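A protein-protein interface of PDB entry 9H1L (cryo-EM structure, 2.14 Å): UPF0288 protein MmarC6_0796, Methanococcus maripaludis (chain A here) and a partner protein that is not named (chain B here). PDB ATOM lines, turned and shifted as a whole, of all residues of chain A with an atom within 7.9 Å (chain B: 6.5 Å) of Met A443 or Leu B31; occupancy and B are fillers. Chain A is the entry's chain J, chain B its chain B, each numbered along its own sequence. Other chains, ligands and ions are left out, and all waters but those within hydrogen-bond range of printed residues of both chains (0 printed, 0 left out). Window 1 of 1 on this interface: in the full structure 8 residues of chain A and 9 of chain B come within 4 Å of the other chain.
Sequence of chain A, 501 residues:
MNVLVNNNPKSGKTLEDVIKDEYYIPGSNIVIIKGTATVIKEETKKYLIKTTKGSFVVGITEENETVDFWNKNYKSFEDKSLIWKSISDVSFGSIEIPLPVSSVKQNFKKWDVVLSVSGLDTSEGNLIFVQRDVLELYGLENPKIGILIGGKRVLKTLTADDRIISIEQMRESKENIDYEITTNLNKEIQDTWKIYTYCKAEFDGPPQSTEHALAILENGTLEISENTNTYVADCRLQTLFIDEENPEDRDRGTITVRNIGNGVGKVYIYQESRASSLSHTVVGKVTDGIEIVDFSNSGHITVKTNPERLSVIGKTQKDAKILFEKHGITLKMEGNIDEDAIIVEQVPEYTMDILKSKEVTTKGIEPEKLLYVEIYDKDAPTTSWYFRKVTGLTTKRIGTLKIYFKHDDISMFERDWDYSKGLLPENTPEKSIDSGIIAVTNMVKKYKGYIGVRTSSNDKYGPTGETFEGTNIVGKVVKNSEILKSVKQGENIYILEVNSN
Among the printed residues, pairs that only touch across the chains: Leu A424 with Lys B213 (3.6 Å), Pro A425 with Lys B30 (3.98 Å), Pro A425 with Leu B31 (3.7 Å), Met A443 with Glu B207 (3.4 Å), Val A444 with Lys B30 (3.3 Å), Val A444 with Leu B31 (3.7 Å) and Val A444 with Arg B32 (3.4 Å).
Met A443 touches just these residues of chain B: Leu B31 (3.5 Å) and Glu B207 (3.4 Å).
Of the printed residues of chain B, Lys A448 touches His B187 (2.9 Å) and Glu B207 (3.6 Å).
Of the printed residues of chain B, Glu A469 touches Lys B30 (3.6 Å).
Leu B31 touches three residues of chain A.
Of the printed residues of chain A, Glu B33 touches Val A444.
Of the printed residues of chain A, His B187 touches Lys A448.
Printed residues of chain A within 4 Å of Lys B213: Leu A424.
The nearest printed residue of chain A that does not touch His B187 is Ser A420 (5.9 Å).
The side-chain carboxylate (OE2) of Glu B207 sits close to the backbone carbonyl oxygen (O) of Lys A421, at 2.6 Å.
The backbone NH of Glu B33 is in hydrogen-bond range of the backbone carbonyl oxygen of Val A444 (3.0 Å).
NZ of Lys A448 sits at hydrogen-bond distance from NE2 of His B187 (2.9 Å).
The side-chain amino group of Lys A448 is in salt-bridge range of the side-chain carboxylate of Glu B207 (3.6 Å).
OE2 of Glu A469 lies within salt-bridge range of NZ of Lys B30 (3.99 Å).
The backbone carbonyl oxygen (O) of Leu B31 lies close to the side-chain sulfur (SD) of Met A443, 3.5 Å away.
The backbone carbonyl oxygen of Leu A423 lies close to the backbone NH of Met A443 (3.1 Å).
The side-chain amide oxygen of Asn A442 lies close to the backbone NH of Val A444 (3.3 Å).
The side-chain amino group (NZ) of Lys B30 is in salt-bridge range of the side-chain carboxylate (OE1) of Glu B33 (2.9 Å).
O of Thr B144 sits at hydrogen-bond distance from NH1 of Arg B32, at 2.7 Å.
NH2 of Arg B32 sits at hydrogen-bond distance from O of Phe B147, at 2.7 Å.
Printed residues of chain B that touch a printed residue of chain A: Lys B30, Leu B31, Arg B32, Glu B33, His B187, Glu B207 and Lys B213.
Hydrophobic or aromatic side chains of chain B within 4 Å of the printed part of chain A: Leu B31 and His B187.
Hydrophobic or aromatic side chains of chain A that line the printed part of chain B: Leu A424, Pro A425, Met A443 and Val A444.
Among the printed residues, 13 pairs touch across the chains.
Among the printed residues, Asp or Glu carboxylates within 4 Å of a Lys or Arg side-chain nitrogen of the other chain: Lys A448 with Glu B207 (3.6 Å) and Glu A469 with Lys B30 (3.99 Å).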
ATOM      1  N   SER A 420      -6.506  -1.414  -5.059  1.00  0.00           N
ATOM      2  CA  SER A 420      -6.534  -1.571  -6.510  1.00  0.00           C
ATOM      3  C   SER A 420      -5.850  -0.372  -7.164  1.00  0.00           C
ATOM      4  O   SER A 420      -6.477   0.502  -7.764  1.00  0.00           O
ATOM      5  CB  SER A 420      -7.968  -1.730  -6.996  1.00  0.00           C
ATOM      6  OG  SER A 420      -8.809  -0.739  -6.430  1.00  0.00           O
ATOM      7  N   LYS A 421      -4.525  -0.342  -7.035  1.00  0.00           N
ATOM      8  CA  LYS A 421      -3.718   0.740  -7.584  1.00  0.00           C
ATOM      9  C   LYS A 421      -2.803   0.264  -8.704  1.00  0.00           C
ATOM     10  O   LYS A 421      -2.875   0.776  -9.824  1.00  0.00           O
ATOM     11  CB  LYS A 421      -2.902   1.400  -6.467  1.00  0.00           C
ATOM     12  CG  LYS A 421      -3.720   1.776  -5.245  1.00  0.00           C
ATOM     13  CD  LYS A 421      -4.880   2.688  -5.609  1.00  0.00           C
ATOM     14  CE  LYS A 421      -4.441   4.141  -5.663  1.00  0.00           C
ATOM     15  NZ  LYS A 421      -4.799   4.870  -4.418  1.00  0.00           N
ATOM     16  N   GLY A 422      -1.948  -0.717  -8.441  1.00  0.00           N
ATOM     17  CA  GLY A 422      -1.022  -1.180  -9.452  1.00  0.00           C
ATOM     18  C   GLY A 422      -1.545  -2.362 -10.239  1.00  0.00           C
ATOM     19  O   GLY A 422      -0.786  -3.277 -10.571  1.00  0.00           O
ATOM     20  N   LEU A 423      -2.841  -2.352 -10.553  1.00  0.00           N
ATOM     21  CA  LEU A 423      -3.481  -3.492 -11.210  1.00  0.00           C
ATOM     22  C   LEU A 423      -3.204  -3.451 -12.712  1.00  0.00           C
ATOM     23  O   LEU A 423      -4.100  -3.332 -13.550  1.00  0.00           O
ATOM     24  CB  LEU A 423      -4.977  -3.503 -10.923  1.00  0.00           C
ATOM     25  CG  LEU A 423      -5.412  -4.101  -9.588  1.00  0.00           C
ATOM     26  CD1 LEU A 423      -6.923  -4.081  -9.474  1.00  0.00           C
ATOM     27  CD2 LEU A 423      -4.876  -5.508  -9.421  1.00  0.00           C
ATOM     28  N   LEU A 424      -1.924  -3.561 -13.049  1.00  0.00           N
ATOM     29  CA  LEU A 424      -1.535  -3.681 -14.442  1.00  0.00           C
ATOM     30  C   LEU A 424      -2.051  -5.002 -15.011  1.00  0.00           C
ATOM     31  O   LEU A 424      -2.189  -5.986 -14.280  1.00  0.00           O
ATOM     32  CB  LEU A 424      -0.016  -3.622 -14.580  1.00  0.00           C
ATOM     33  CG  LEU A 424       0.680  -2.284 -14.337  1.00  0.00           C
ATOM     34  CD1 LEU A 424       2.152  -2.394 -14.684  1.00  0.00           C
ATOM     35  CD2 LEU A 424       0.027  -1.181 -15.145  1.00  0.00           C
ATOM     36  N   PRO A 425      -2.357  -5.047 -16.308  1.00  0.00           N
ATOM     37  CA  PRO A 425      -2.763  -6.319 -16.918  1.00  0.00           C
ATOM     38  C   PRO A 425      -1.691  -7.383 -16.744  1.00  0.00           C
ATOM     39  O   PRO A 425      -0.597  -7.265 -17.301  1.00  0.00           O
ATOM     40  CB  PRO A 425      -2.965  -5.955 -18.394  1.00  0.00           C
ATOM     41  CG  PRO A 425      -3.233  -4.494 -18.389  1.00  0.00           C
ATOM     42  CD  PRO A 425      -2.442  -3.922 -17.255  1.00  0.00           C
ATOM     43  N   VAL A 440     -10.054 -10.594 -11.846  1.00  0.00           N
ATOM     44  CA  VAL A 440     -10.161  -9.198 -11.447  1.00  0.00           C
ATOM     45  C   VAL A 440      -9.913  -8.330 -12.671  1.00  0.00           C
ATOM     46  O   VAL A 440      -8.975  -8.565 -13.440  1.00  0.00           O
ATOM     47  CB  VAL A 440      -9.170  -8.836 -10.318  1.00  0.00           C
ATOM     48  CG1 VAL A 440      -9.559  -7.523  -9.673  1.00  0.00           C
ATOM     49  CG2 VAL A 440      -9.113  -9.945  -9.282  1.00  0.00           C
ATOM     50  N   THR A 441     -10.763  -7.326 -12.857  1.00  0.00           N
ATOM     51  CA  THR A 441     -10.606  -6.388 -13.959  1.00  0.00           C
ATOM     52  C   THR A 441      -9.476  -5.418 -13.637  1.00  0.00           C
ATOM     53  O   THR A 441      -9.440  -4.839 -12.548  1.00  0.00           O
ATOM     54  CB  THR A 441     -11.902  -5.621 -14.216  1.00  0.00           C
ATOM     55  OG1 THR A 441     -11.896  -4.409 -13.457  1.00  0.00           O
ATOM     56  CG2 THR A 441     -13.092  -6.448 -13.792  1.00  0.00           C
ATOM     57  N   ASN A 442      -8.557  -5.246 -14.583  1.00  0.00           N
ATOM     58  CA  ASN A 442      -7.386  -4.406 -14.369  1.00  0.00           C
ATOM     59  C   ASN A 442      -7.756  -2.937 -14.576  1.00  0.00           C
ATOM     60  O   ASN A 442      -8.924  -2.581 -14.755  1.00  0.00           O
ATOM     61  CB  ASN A 442      -6.247  -4.848 -15.281  1.00  0.00           C
ATOM     62  CG  ASN A 442      -6.711  -5.156 -16.684  1.00  0.00           C
ATOM     63  OD1 ASN A 442      -7.497  -4.411 -17.263  1.00  0.00           O
ATOM     64  ND2 ASN A 442      -6.218  -6.251 -17.243  1.00  0.00           N
ATOM     65  N   MET A 443      -6.750  -2.063 -14.568  1.00  0.00           N
ATOM     66  CA  MET A 443      -6.967  -0.627 -14.681  1.00  0.00           C
ATOM     67  C   MET A 443      -7.422  -0.200 -16.067  1.00  0.00           C
ATOM     68  O   MET A 443      -7.786   0.967 -16.248  1.00  0.00           O
ATOM     69  CB  MET A 443      -5.687   0.130 -14.321  1.00  0.00           C
ATOM     70  CG  MET A 443      -4.421  -0.537 -14.817  1.00  0.00           C
ATOM     71  SD  MET A 443      -3.127   0.636 -15.256  1.00  0.00           S
ATOM     72  CE  MET A 443      -2.572   1.147 -13.634  1.00  0.00           C
ATOM     73  N   VAL A 444      -7.398  -1.106 -17.046  1.00  0.00           N
ATOM     74  CA  VAL A 444      -7.825  -0.761 -18.397  1.00  0.00           C
ATOM     75  C   VAL A 444      -9.299  -0.380 -18.411  1.00  0.00           C
ATOM     76  O   VAL A 444      -9.698   0.612 -19.032  1.00  0.00           O
ATOM     77  CB  VAL A 444      -7.539  -1.926 -19.358  1.00  0.00           C
ATOM     78  CG1 VAL A 444      -7.917  -1.542 -20.767  1.00  0.00           C
ATOM     79  CG2 VAL A 444      -6.081  -2.319 -19.280  1.00  0.00           C
ATOM     80  N   LYS A 445     -10.127  -1.160 -17.730  1.00  0.00           N
ATOM     81  CA  LYS A 445     -11.562  -0.933 -17.733  1.00  0.00           C
ATOM     82  C   LYS A 445     -11.952   0.089 -16.671  1.00  0.00           C
ATOM     83  O   LYS A 445     -11.172   0.427 -15.778  1.00  0.00           O
ATOM     84  CB  LYS A 445     -12.311  -2.245 -17.508  1.00  0.00           C
ATOM     85  CG  LYS A 445     -11.990  -3.306 -18.541  1.00  0.00           C
ATOM     86  CD  LYS A 445     -12.283  -2.803 -19.943  1.00  0.00           C
ATOM     87  CE  LYS A 445     -12.055  -3.888 -20.977  1.00  0.00           C
ATOM     88  NZ  LYS A 445     -11.605  -3.325 -22.278  1.00  0.00           N
ATOM     89  N   LYS A 446     -13.183   0.587 -16.786  1.00  0.00           N
ATOM     90  CA  LYS A 446     -13.662   1.602 -15.854  1.00  0.00           C
ATOM     91  C   LYS A 446     -13.890   1.013 -14.466  1.00  0.00           C
ATOM     92  O   LYS A 446     -13.645   1.681 -13.455  1.00  0.00           O
ATOM     93  CB  LYS A 446     -14.941   2.237 -16.395  1.00  0.00           C
ATOM     94  CG  LYS A 446     -15.671   3.135 -15.412  1.00  0.00           C
ATOM     95  CD  LYS A 446     -16.962   3.657 -16.018  1.00  0.00           C
ATOM     96  CE  LYS A 446     -16.806   5.090 -16.492  1.00  0.00           C
ATOM     97  NZ  LYS A 446     -17.439   5.298 -17.824  1.00  0.00           N
ATOM     98  N   TYR A 447     -14.355  -0.232 -14.397  1.00  0.00           N
ATOM     99  CA  TYR A 447     -14.613  -0.892 -13.118  1.00  0.00           C
ATOM    100  C   TYR A 447     -13.414  -1.760 -12.738  1.00  0.00           C
ATOM    101  O   TYR A 447     -13.459  -2.990 -12.719  1.00  0.00           O
ATOM    102  CB  TYR A 447     -15.904  -1.696 -13.190  1.00  0.00           C
ATOM    103  CG  TYR A 447     -17.093  -0.828 -13.507  1.00  0.00           C
ATOM    104  CD1 TYR A 447     -17.596   0.053 -12.563  1.00  0.00           C
ATOM    105  CD2 TYR A 447     -17.697  -0.869 -14.753  1.00  0.00           C
ATOM    106  CE1 TYR A 447     -18.671   0.858 -12.843  1.00  0.00           C
ATOM    107  CE2 TYR A 447     -18.777  -0.063 -15.044  1.00  0.00           C
ATOM    108  CZ  TYR A 447     -19.259   0.798 -14.084  1.00  0.00           C
ATOM    109  OH  TYR A 447     -20.333   1.605 -14.357  1.00  0.00           O
ATOM    110  N   LYS A 448     -12.319  -1.072 -12.423  1.00  0.00           N
ATOM    111  CA  LYS A 448     -11.083  -1.735 -12.038  1.00  0.00           C
ATOM    112  C   LYS A 448     -11.184  -2.233 -10.604  1.00  0.00           C
ATOM    113  O   LYS A 448     -11.640  -1.508  -9.715  1.00  0.00           O
ATOM    114  CB  LYS A 448      -9.901  -0.779 -12.194  1.00  0.00           C
ATOM    115  CG  LYS A 448      -8.712  -1.096 -11.305  1.00  0.00           C
ATOM    116  CD  LYS A 448      -7.849   0.130 -11.080  1.00  0.00           C
ATOM    117  CE  LYS A 448      -8.649   1.253 -10.452  1.00  0.00           C
ATOM    118  NZ  LYS A 448      -7.803   2.432 -10.131  1.00  0.00           N
ATOM    119  N   GLY A 449     -10.766  -3.476 -10.380  1.00  0.00           N
ATOM    120  CA  GLY A 449     -10.708  -4.062  -9.060  1.00  0.00           C
ATOM    121  C   GLY A 449     -11.873  -4.965  -8.714  1.00  0.00           C
ATOM    122  O   GLY A 449     -11.767  -5.745  -7.759  1.00  0.00           O
ATOM    123  N   GLU A 469      -8.756  -8.364 -22.680  1.00  0.00           N
ATOM    124  CA  GLU A 469      -7.652  -7.449 -22.420  1.00  0.00           C
ATOM    125  C   GLU A 469      -7.850  -6.653 -21.137  1.00  0.00           C
ATOM    126  O   GLU A 469      -6.878  -6.106 -20.608  1.00  0.00           O
ATOM    127  CB  GLU A 469      -7.461  -6.499 -23.602  1.00  0.00           C
ATOM    128  CG  GLU A 469      -8.157  -5.161 -23.452  1.00  0.00           C
ATOM    129  CD  GLU A 469      -9.490  -5.121 -24.164  1.00  0.00           C
ATOM    130  OE1 GLU A 469      -9.820  -6.100 -24.865  1.00  0.00           O
ATOM    131  OE2 GLU A 469     -10.209  -4.108 -24.024  1.00  0.00           O
ATOM    132  N   GLY A 470      -9.075  -6.576 -20.628  1.00  0.00           N
ATOM    133  CA  GLY A 470      -9.370  -5.894 -19.386  1.00  0.00           C
ATOM    134  C   GLY A 470      -9.558  -6.796 -18.188  1.00  0.00           C
ATOM    135  O   GLY A 470     -10.084  -6.340 -17.165  1.00  0.00           O
ATOM    136  N   THR A 471      -9.150  -8.059 -18.275  1.00  0.00           N
ATOM    137  CA  THR A 471      -9.365  -9.039 -17.220  1.00  0.00           C
ATOM    138  C   THR A 471      -8.080  -9.820 -16.996  1.00  0.00           C
ATOM    139  O   THR A 471      -7.478 -10.311 -17.954  1.00  0.00           O
ATOM    140  CB  THR A 471     -10.510  -9.989 -17.590  1.00  0.00           C
ATOM    141  OG1 THR A 471     -11.766  -9.370 -17.292  1.00  0.00           O
ATOM    142  CG2 THR A 471     -10.399 -11.300 -16.835  1.00  0.00           C
ATOM    143  N   ASN A 472      -7.659  -9.931 -15.737  1.00  0.00           N
ATOM    144  CA  ASN A 472      -6.519 -10.759 -15.373  1.00  0.00           C
ATOM    145  C   ASN A 472      -6.964 -11.857 -14.419  1.00  0.00           C
ATOM    146  O   ASN A 472      -7.585 -11.584 -13.387  1.00  0.00           O
ATOM    147  CB  ASN A 472      -5.382  -9.935 -14.751  1.00  0.00           C
ATOM    148  CG  ASN A 472      -5.878  -8.842 -13.835  1.00  0.00           C
ATOM    149  OD1 ASN A 472      -5.389  -7.715 -13.882  1.00  0.00           O
ATOM    150  ND2 ASN A 472      -6.837  -9.172 -12.982  1.00  0.00           N
ATOM    151  N   GLU B  29       0.103  -2.896 -25.933  1.00  0.00           N
ATOM    152  CA  GLU B  29      -0.712  -3.229 -24.774  1.00  0.00           C
ATOM    153  C   GLU B  29      -1.454  -1.991 -24.296  1.00  0.00           C
ATOM    154  O   GLU B  29      -0.846  -0.941 -24.070  1.00  0.00           O
ATOM    155  CB  GLU B  29       0.164  -3.792 -23.658  1.00  0.00           C
ATOM    156  CG  GLU B  29      -0.483  -3.771 -22.286  1.00  0.00           C
ATOM    157  CD  GLU B  29       0.317  -4.536 -21.255  1.00  0.00           C
ATOM    158  OE1 GLU B  29       0.343  -5.782 -21.324  1.00  0.00           O
ATOM    159  OE2 GLU B  29       0.923  -3.893 -20.374  1.00  0.00           O
ATOM    160  N   LYS B  30      -2.771  -2.107 -24.149  1.00  0.00           N
ATOM    161  CA  LYS B  30      -3.572  -0.993 -23.674  1.00  0.00           C
ATOM    162  C   LYS B  30      -3.648  -1.023 -22.156  1.00  0.00           C
ATOM    163  O   LYS B  30      -3.643  -2.088 -21.535  1.00  0.00           O
ATOM    164  CB  LYS B  30      -4.965  -1.006 -24.311  1.00  0.00           C
ATOM    165  CG  LYS B  30      -5.933  -2.041 -23.787  1.00  0.00           C
ATOM    166  CD  LYS B  30      -7.336  -1.767 -24.308  1.00  0.00           C
ATOM    167  CE  LYS B  30      -7.776  -0.342 -24.027  1.00  0.00           C
ATOM    168  NZ  LYS B  30      -9.252  -0.242 -23.862  1.00  0.00           N
ATOM    169  N   LEU B  31      -3.672   0.168 -21.557  1.00  0.00           N
ATOM    170  CA  LEU B  31      -3.579   0.315 -20.113  1.00  0.00           C
ATOM    171  C   LEU B  31      -4.676   1.180 -19.515  1.00  0.00           C
ATOM    172  O   LEU B  31      -4.719   1.325 -18.290  1.00  0.00           O
ATOM    173  CB  LEU B  31      -2.217   0.912 -19.724  1.00  0.00           C
ATOM    174  CG  LEU B  31      -0.983   0.096 -20.116  1.00  0.00           C
ATOM    175  CD1 LEU B  31       0.288   0.897 -19.900  1.00  0.00           C
ATOM    176  CD2 LEU B  31      -0.932  -1.207 -19.342  1.00  0.00           C
ATOM    177  N   ARG B  32      -5.553   1.756 -20.331  1.00  0.00           N
ATOM    178  CA  ARG B  32      -6.619   2.619 -19.846  1.00  0.00           C
ATOM    179  C   ARG B  32      -7.720   2.639 -20.891  1.00  0.00           C
ATOM    180  O   ARG B  32      -7.507   2.263 -22.045  1.00  0.00           O
ATOM    181  CB  ARG B  32      -6.108   4.035 -19.573  1.00  0.00           C
ATOM    182  CG  ARG B  32      -5.481   4.683 -20.794  1.00  0.00           C
ATOM    183  CD  ARG B  32      -4.558   5.826 -20.433  1.00  0.00           C
ATOM    184  NE  ARG B  32      -3.350   5.370 -19.758  1.00  0.00           N
ATOM    185  CZ  ARG B  32      -2.270   4.921 -20.380  1.00  0.00           C
ATOM    186  NH1 ARG B  32      -2.210   4.852 -21.698  1.00  0.00           N
ATOM    187  NH2 ARG B  32      -1.222   4.532 -19.659  1.00  0.00           N
ATOM    188  N   GLU B  33      -8.902   3.084 -20.475  1.00  0.00           N
ATOM    189  CA  GLU B  33     -10.012   3.306 -21.393  1.00  0.00           C
ATOM    190  C   GLU B  33     -10.448   4.759 -21.266  1.00  0.00           C
ATOM    191  O   GLU B  33     -11.059   5.147 -20.264  1.00  0.00           O
ATOM    192  CB  GLU B  33     -11.178   2.359 -21.115  1.00  0.00           C
ATOM    193  CG  GLU B  33     -12.442   2.682 -21.897  1.00  0.00           C
ATOM    194  CD  GLU B  33     -12.299   2.418 -23.383  1.00  0.00           C
ATOM    195  OE1 GLU B  33     -11.498   1.536 -23.757  1.00  0.00           O
ATOM    196  OE2 GLU B  33     -12.989   3.094 -24.173  1.00  0.00           O
ATOM    197  N   ASP B 143      -4.715   5.282 -25.265  1.00  0.00           N
ATOM    198  CA  ASP B 143      -5.109   4.173 -24.410  1.00  0.00           C
ATOM    199  C   ASP B 143      -4.047   3.088 -24.279  1.00  0.00           C
ATOM    200  O   ASP B 143      -4.177   2.223 -23.410  1.00  0.00           O
ATOM    201  CB  ASP B 143      -6.416   3.552 -24.917  1.00  0.00           C
ATOM    202  CG  ASP B 143      -6.239   2.802 -26.220  1.00  0.00           C
ATOM    203  OD1 ASP B 143      -5.349   3.180 -27.010  1.00  0.00           O
ATOM    204  OD2 ASP B 143      -6.993   1.836 -26.459  1.00  0.00           O
ATOM    205  N   THR B 144      -3.004   3.114 -25.100  1.00  0.00           N
ATOM    206  CA  THR B 144      -2.025   2.040 -25.138  1.00  0.00           C
ATOM    207  C   THR B 144      -0.838   2.365 -24.236  1.00  0.00           C
ATOM    208  O   THR B 144      -0.863   3.321 -23.454  1.00  0.00           O
ATOM    209  CB  THR B 144      -1.566   1.781 -26.573  1.00  0.00           C
ATOM    210  OG1 THR B 144      -1.095   3.002 -27.153  1.00  0.00           O
ATOM    211  CG2 THR B 144      -2.705   1.229 -27.408  1.00  0.00           C
ATOM    212  N   GLU B 145       0.213   1.557 -24.351  1.00  0.00           N
ATOM    213  CA  GLU B 145       1.455   1.752 -23.616  1.00  0.00           C
ATOM    214  C   GLU B 145       2.333   2.845 -24.211  1.00  0.00           C
ATOM    215  O   GLU B 145       3.450   3.041 -23.733  1.00  0.00           O
ATOM    216  CB  GLU B 145       2.237   0.438 -23.552  1.00  0.00           C
ATOM    217  CG  GLU B 145       2.618  -0.122 -24.911  1.00  0.00           C
ATOM    218  CD  GLU B 145       3.189  -1.520 -24.822  1.00  0.00           C
ATOM    219  OE1 GLU B 145       3.468  -1.978 -23.694  1.00  0.00           O
ATOM    220  OE2 GLU B 145       3.360  -2.163 -25.878  1.00  0.00           O
ATOM    221  N   LEU B 146       1.867   3.540 -25.248  1.00  0.00           N
ATOM    222  CA  LEU B 146       2.555   4.715 -25.756  1.00  0.00           C
ATOM    223  C   LEU B 146       2.311   5.950 -24.903  1.00  0.00           C
ATOM    224  O   LEU B 146       3.009   6.953 -25.077  1.00  0.00           O
ATOM    225  CB  LEU B 146       2.107   5.007 -27.191  1.00  0.00           C
ATOM    226  CG  LEU B 146       3.110   4.750 -28.313  1.00  0.00           C
ATOM    227  CD1 LEU B 146       3.558   3.305 -28.295  1.00  0.00           C
ATOM    228  CD2 LEU B 146       2.495   5.107 -29.653  1.00  0.00           C
ATOM    229  N   PHE B 147       1.344   5.901 -23.994  1.00  0.00           N
ATOM    230  CA  PHE B 147       0.948   7.056 -23.204  1.00  0.00           C
ATOM    231  C   PHE B 147       1.029   6.723 -21.724  1.00  0.00           C
ATOM    232  O   PHE B 147       0.657   5.626 -21.301  1.00  0.00           O
ATOM    233  CB  PHE B 147      -0.472   7.501 -23.562  1.00  0.00           C
ATOM    234  CG  PHE B 147      -0.943   8.705 -22.802  1.00  0.00           C
ATOM    235  CD1 PHE B 147      -0.338   9.937 -22.984  1.00  0.00           C
ATOM    236  CD2 PHE B 147      -1.996   8.606 -21.909  1.00  0.00           C
ATOM    237  CE1 PHE B 147      -0.772  11.046 -22.285  1.00  0.00           C
ATOM    238  CE2 PHE B 147      -2.435   9.713 -21.206  1.00  0.00           C
ATOM    239  CZ  PHE B 147      -1.821  10.932 -21.395  1.00  0.00           C
ATOM    240  N   HIS B 187      -5.882   9.011  -9.505  1.00  0.00           N
ATOM    241  CA  HIS B 187      -5.915   9.129 -10.953  1.00  0.00           C
ATOM    242  C   HIS B 187      -5.523  10.535 -11.381  1.00  0.00           C
ATOM    243  O   HIS B 187      -5.664  11.502 -10.629  1.00  0.00           O
ATOM    244  CB  HIS B 187      -7.307   8.800 -11.503  1.00  0.00           C
ATOM    245  CG  HIS B 187      -7.635   7.341 -11.493  1.00  0.00           C
ATOM    246  ND1 HIS B 187      -8.714   6.820 -12.174  1.00  0.00           N
ATOM    247  CD2 HIS B 187      -7.035   6.296 -10.883  1.00  0.00           C
ATOM    248  CE1 HIS B 187      -8.760   5.513 -11.986  1.00  0.00           C
ATOM    249  NE2 HIS B 187      -7.751   5.170 -11.206  1.00  0.00           N
ATOM    250  N   GLY B 206      -6.759   8.241 -16.326  1.00  0.00           N
ATOM    251  CA  GLY B 206      -6.255   7.065 -15.665  1.00  0.00           C
ATOM    252  C   GLY B 206      -5.208   7.437 -14.643  1.00  0.00           C
ATOM    253  O   GLY B 206      -4.955   8.611 -14.380  1.00  0.00           O
ATOM    254  N   GLU B 207      -4.598   6.427 -14.074  1.00  0.00           N
ATOM    255  CA  GLU B 207      -3.598   6.589 -13.037  1.00  0.00           C
ATOM    256  C   GLU B 207      -2.196   6.519 -13.626  1.00  0.00           C
ATOM    257  O   GLU B 207      -1.998   5.985 -14.722  1.00  0.00           O
ATOM    258  CB  GLU B 207      -3.786   5.516 -11.964  1.00  0.00           C
ATOM    259  CG  GLU B 207      -3.092   4.210 -12.234  1.00  0.00           C
ATOM    260  CD  GLU B 207      -3.159   3.295 -11.043  1.00  0.00           C
ATOM    261  OE1 GLU B 207      -4.240   2.723 -10.803  1.00  0.00           O
ATOM    262  OE2 GLU B 207      -2.135   3.162 -10.338  1.00  0.00           O
ATOM    263  N   PRO B 208      -1.206   7.105 -12.947  1.00  0.00           N
ATOM    264  CA  PRO B 208       0.178   7.009 -13.435  1.00  0.00           C
ATOM    265  C   PRO B 208       0.679   5.576 -13.482  1.00  0.00           C
ATOM    266  O   PRO B 208       0.359   4.752 -12.622  1.00  0.00           O
ATOM    267  CB  PRO B 208       0.975   7.841 -12.423  1.00  0.00           C
ATOM    268  CG  PRO B 208       0.017   8.275 -11.368  1.00  0.00           C
ATOM    269  CD  PRO B 208      -1.354   8.135 -11.908  1.00  0.00           C
ATOM    270  N   ILE B 209       1.468   5.285 -14.508  1.00  0.00           N
ATOM    271  CA  ILE B 209       2.123   3.978 -14.625  1.00  0.00           C
ATOM    272  C   ILE B 209       3.184   3.858 -13.539  1.00  0.00           C
ATOM    273  O   ILE B 209       3.919   4.831 -13.294  1.00  0.00           O
ATOM    274  CB  ILE B 209       2.736   3.816 -16.021  1.00  0.00           C
ATOM    275  CG1 ILE B 209       1.686   4.055 -17.104  1.00  0.00           C
ATOM    276  CG2 ILE B 209       3.353   2.439 -16.199  1.00  0.00           C
ATOM    277  CD1 ILE B 209       0.451   3.198 -16.964  1.00  0.00           C
ATOM    278  N   PRO B 210       3.282   2.724 -12.839  1.00  0.00           N
ATOM    279  CA  PRO B 210       4.353   2.558 -11.851  1.00  0.00           C
ATOM    280  C   PRO B 210       5.725   2.586 -12.504  1.00  0.00           C
ATOM    281  O   PRO B 210       5.885   2.240 -13.676  1.00  0.00           O
ATOM    282  CB  PRO B 210       4.057   1.185 -11.232  1.00  0.00           C
ATOM    283  CG  PRO B 210       2.608   0.966 -11.479  1.00  0.00           C
ATOM    284  CD  PRO B 210       2.314   1.616 -12.794  1.00  0.00           C
ATOM    285  N   LYS B 213       7.236  -0.623 -14.176  1.00  0.00           N
ATOM    286  CA  LYS B 213       6.759  -0.850 -15.536  1.00  0.00           C
ATOM    287  C   LYS B 213       7.342   0.173 -16.506  1.00  0.00           C
ATOM    288  O   LYS B 213       7.629  -0.160 -17.665  1.00  0.00           O
ATOM    289  CB  LYS B 213       5.227  -0.813 -15.556  1.00  0.00           C
ATOM    290  CG  LYS B 213       4.594  -0.989 -16.925  1.00  0.00           C
ATOM    291  CD  LYS B 213       4.684  -2.427 -17.397  1.00  0.00           C
ATOM    292  CE  LYS B 213       3.671  -2.711 -18.489  1.00  0.00           C
ATOM    293  NZ  LYS B 213       3.660  -4.146 -18.868  1.00  0.00           N
ATOM    294  N   ILE B 217       9.042  -0.371 -20.251  1.00  0.00           N
ATOM    295  CA  ILE B 217       8.352   0.048 -21.468  1.00  0.00           C
ATOM    296  C   ILE B 217       8.912   1.333 -22.065  1.00  0.00           C
ATOM    297  O   ILE B 217       8.378   1.812 -23.075  1.00  0.00           O
ATOM    298  CB  ILE B 217       6.836   0.200 -21.224  1.00  0.00           C
ATOM    299  CG1 ILE B 217       6.547   1.415 -20.340  1.00  0.00           C
ATOM    300  CG2 ILE B 217       6.269  -1.063 -20.611  1.00  0.00           C
ATOM    301  CD1 ILE B 217       5.078   1.668 -20.123  1.00  0.00           C
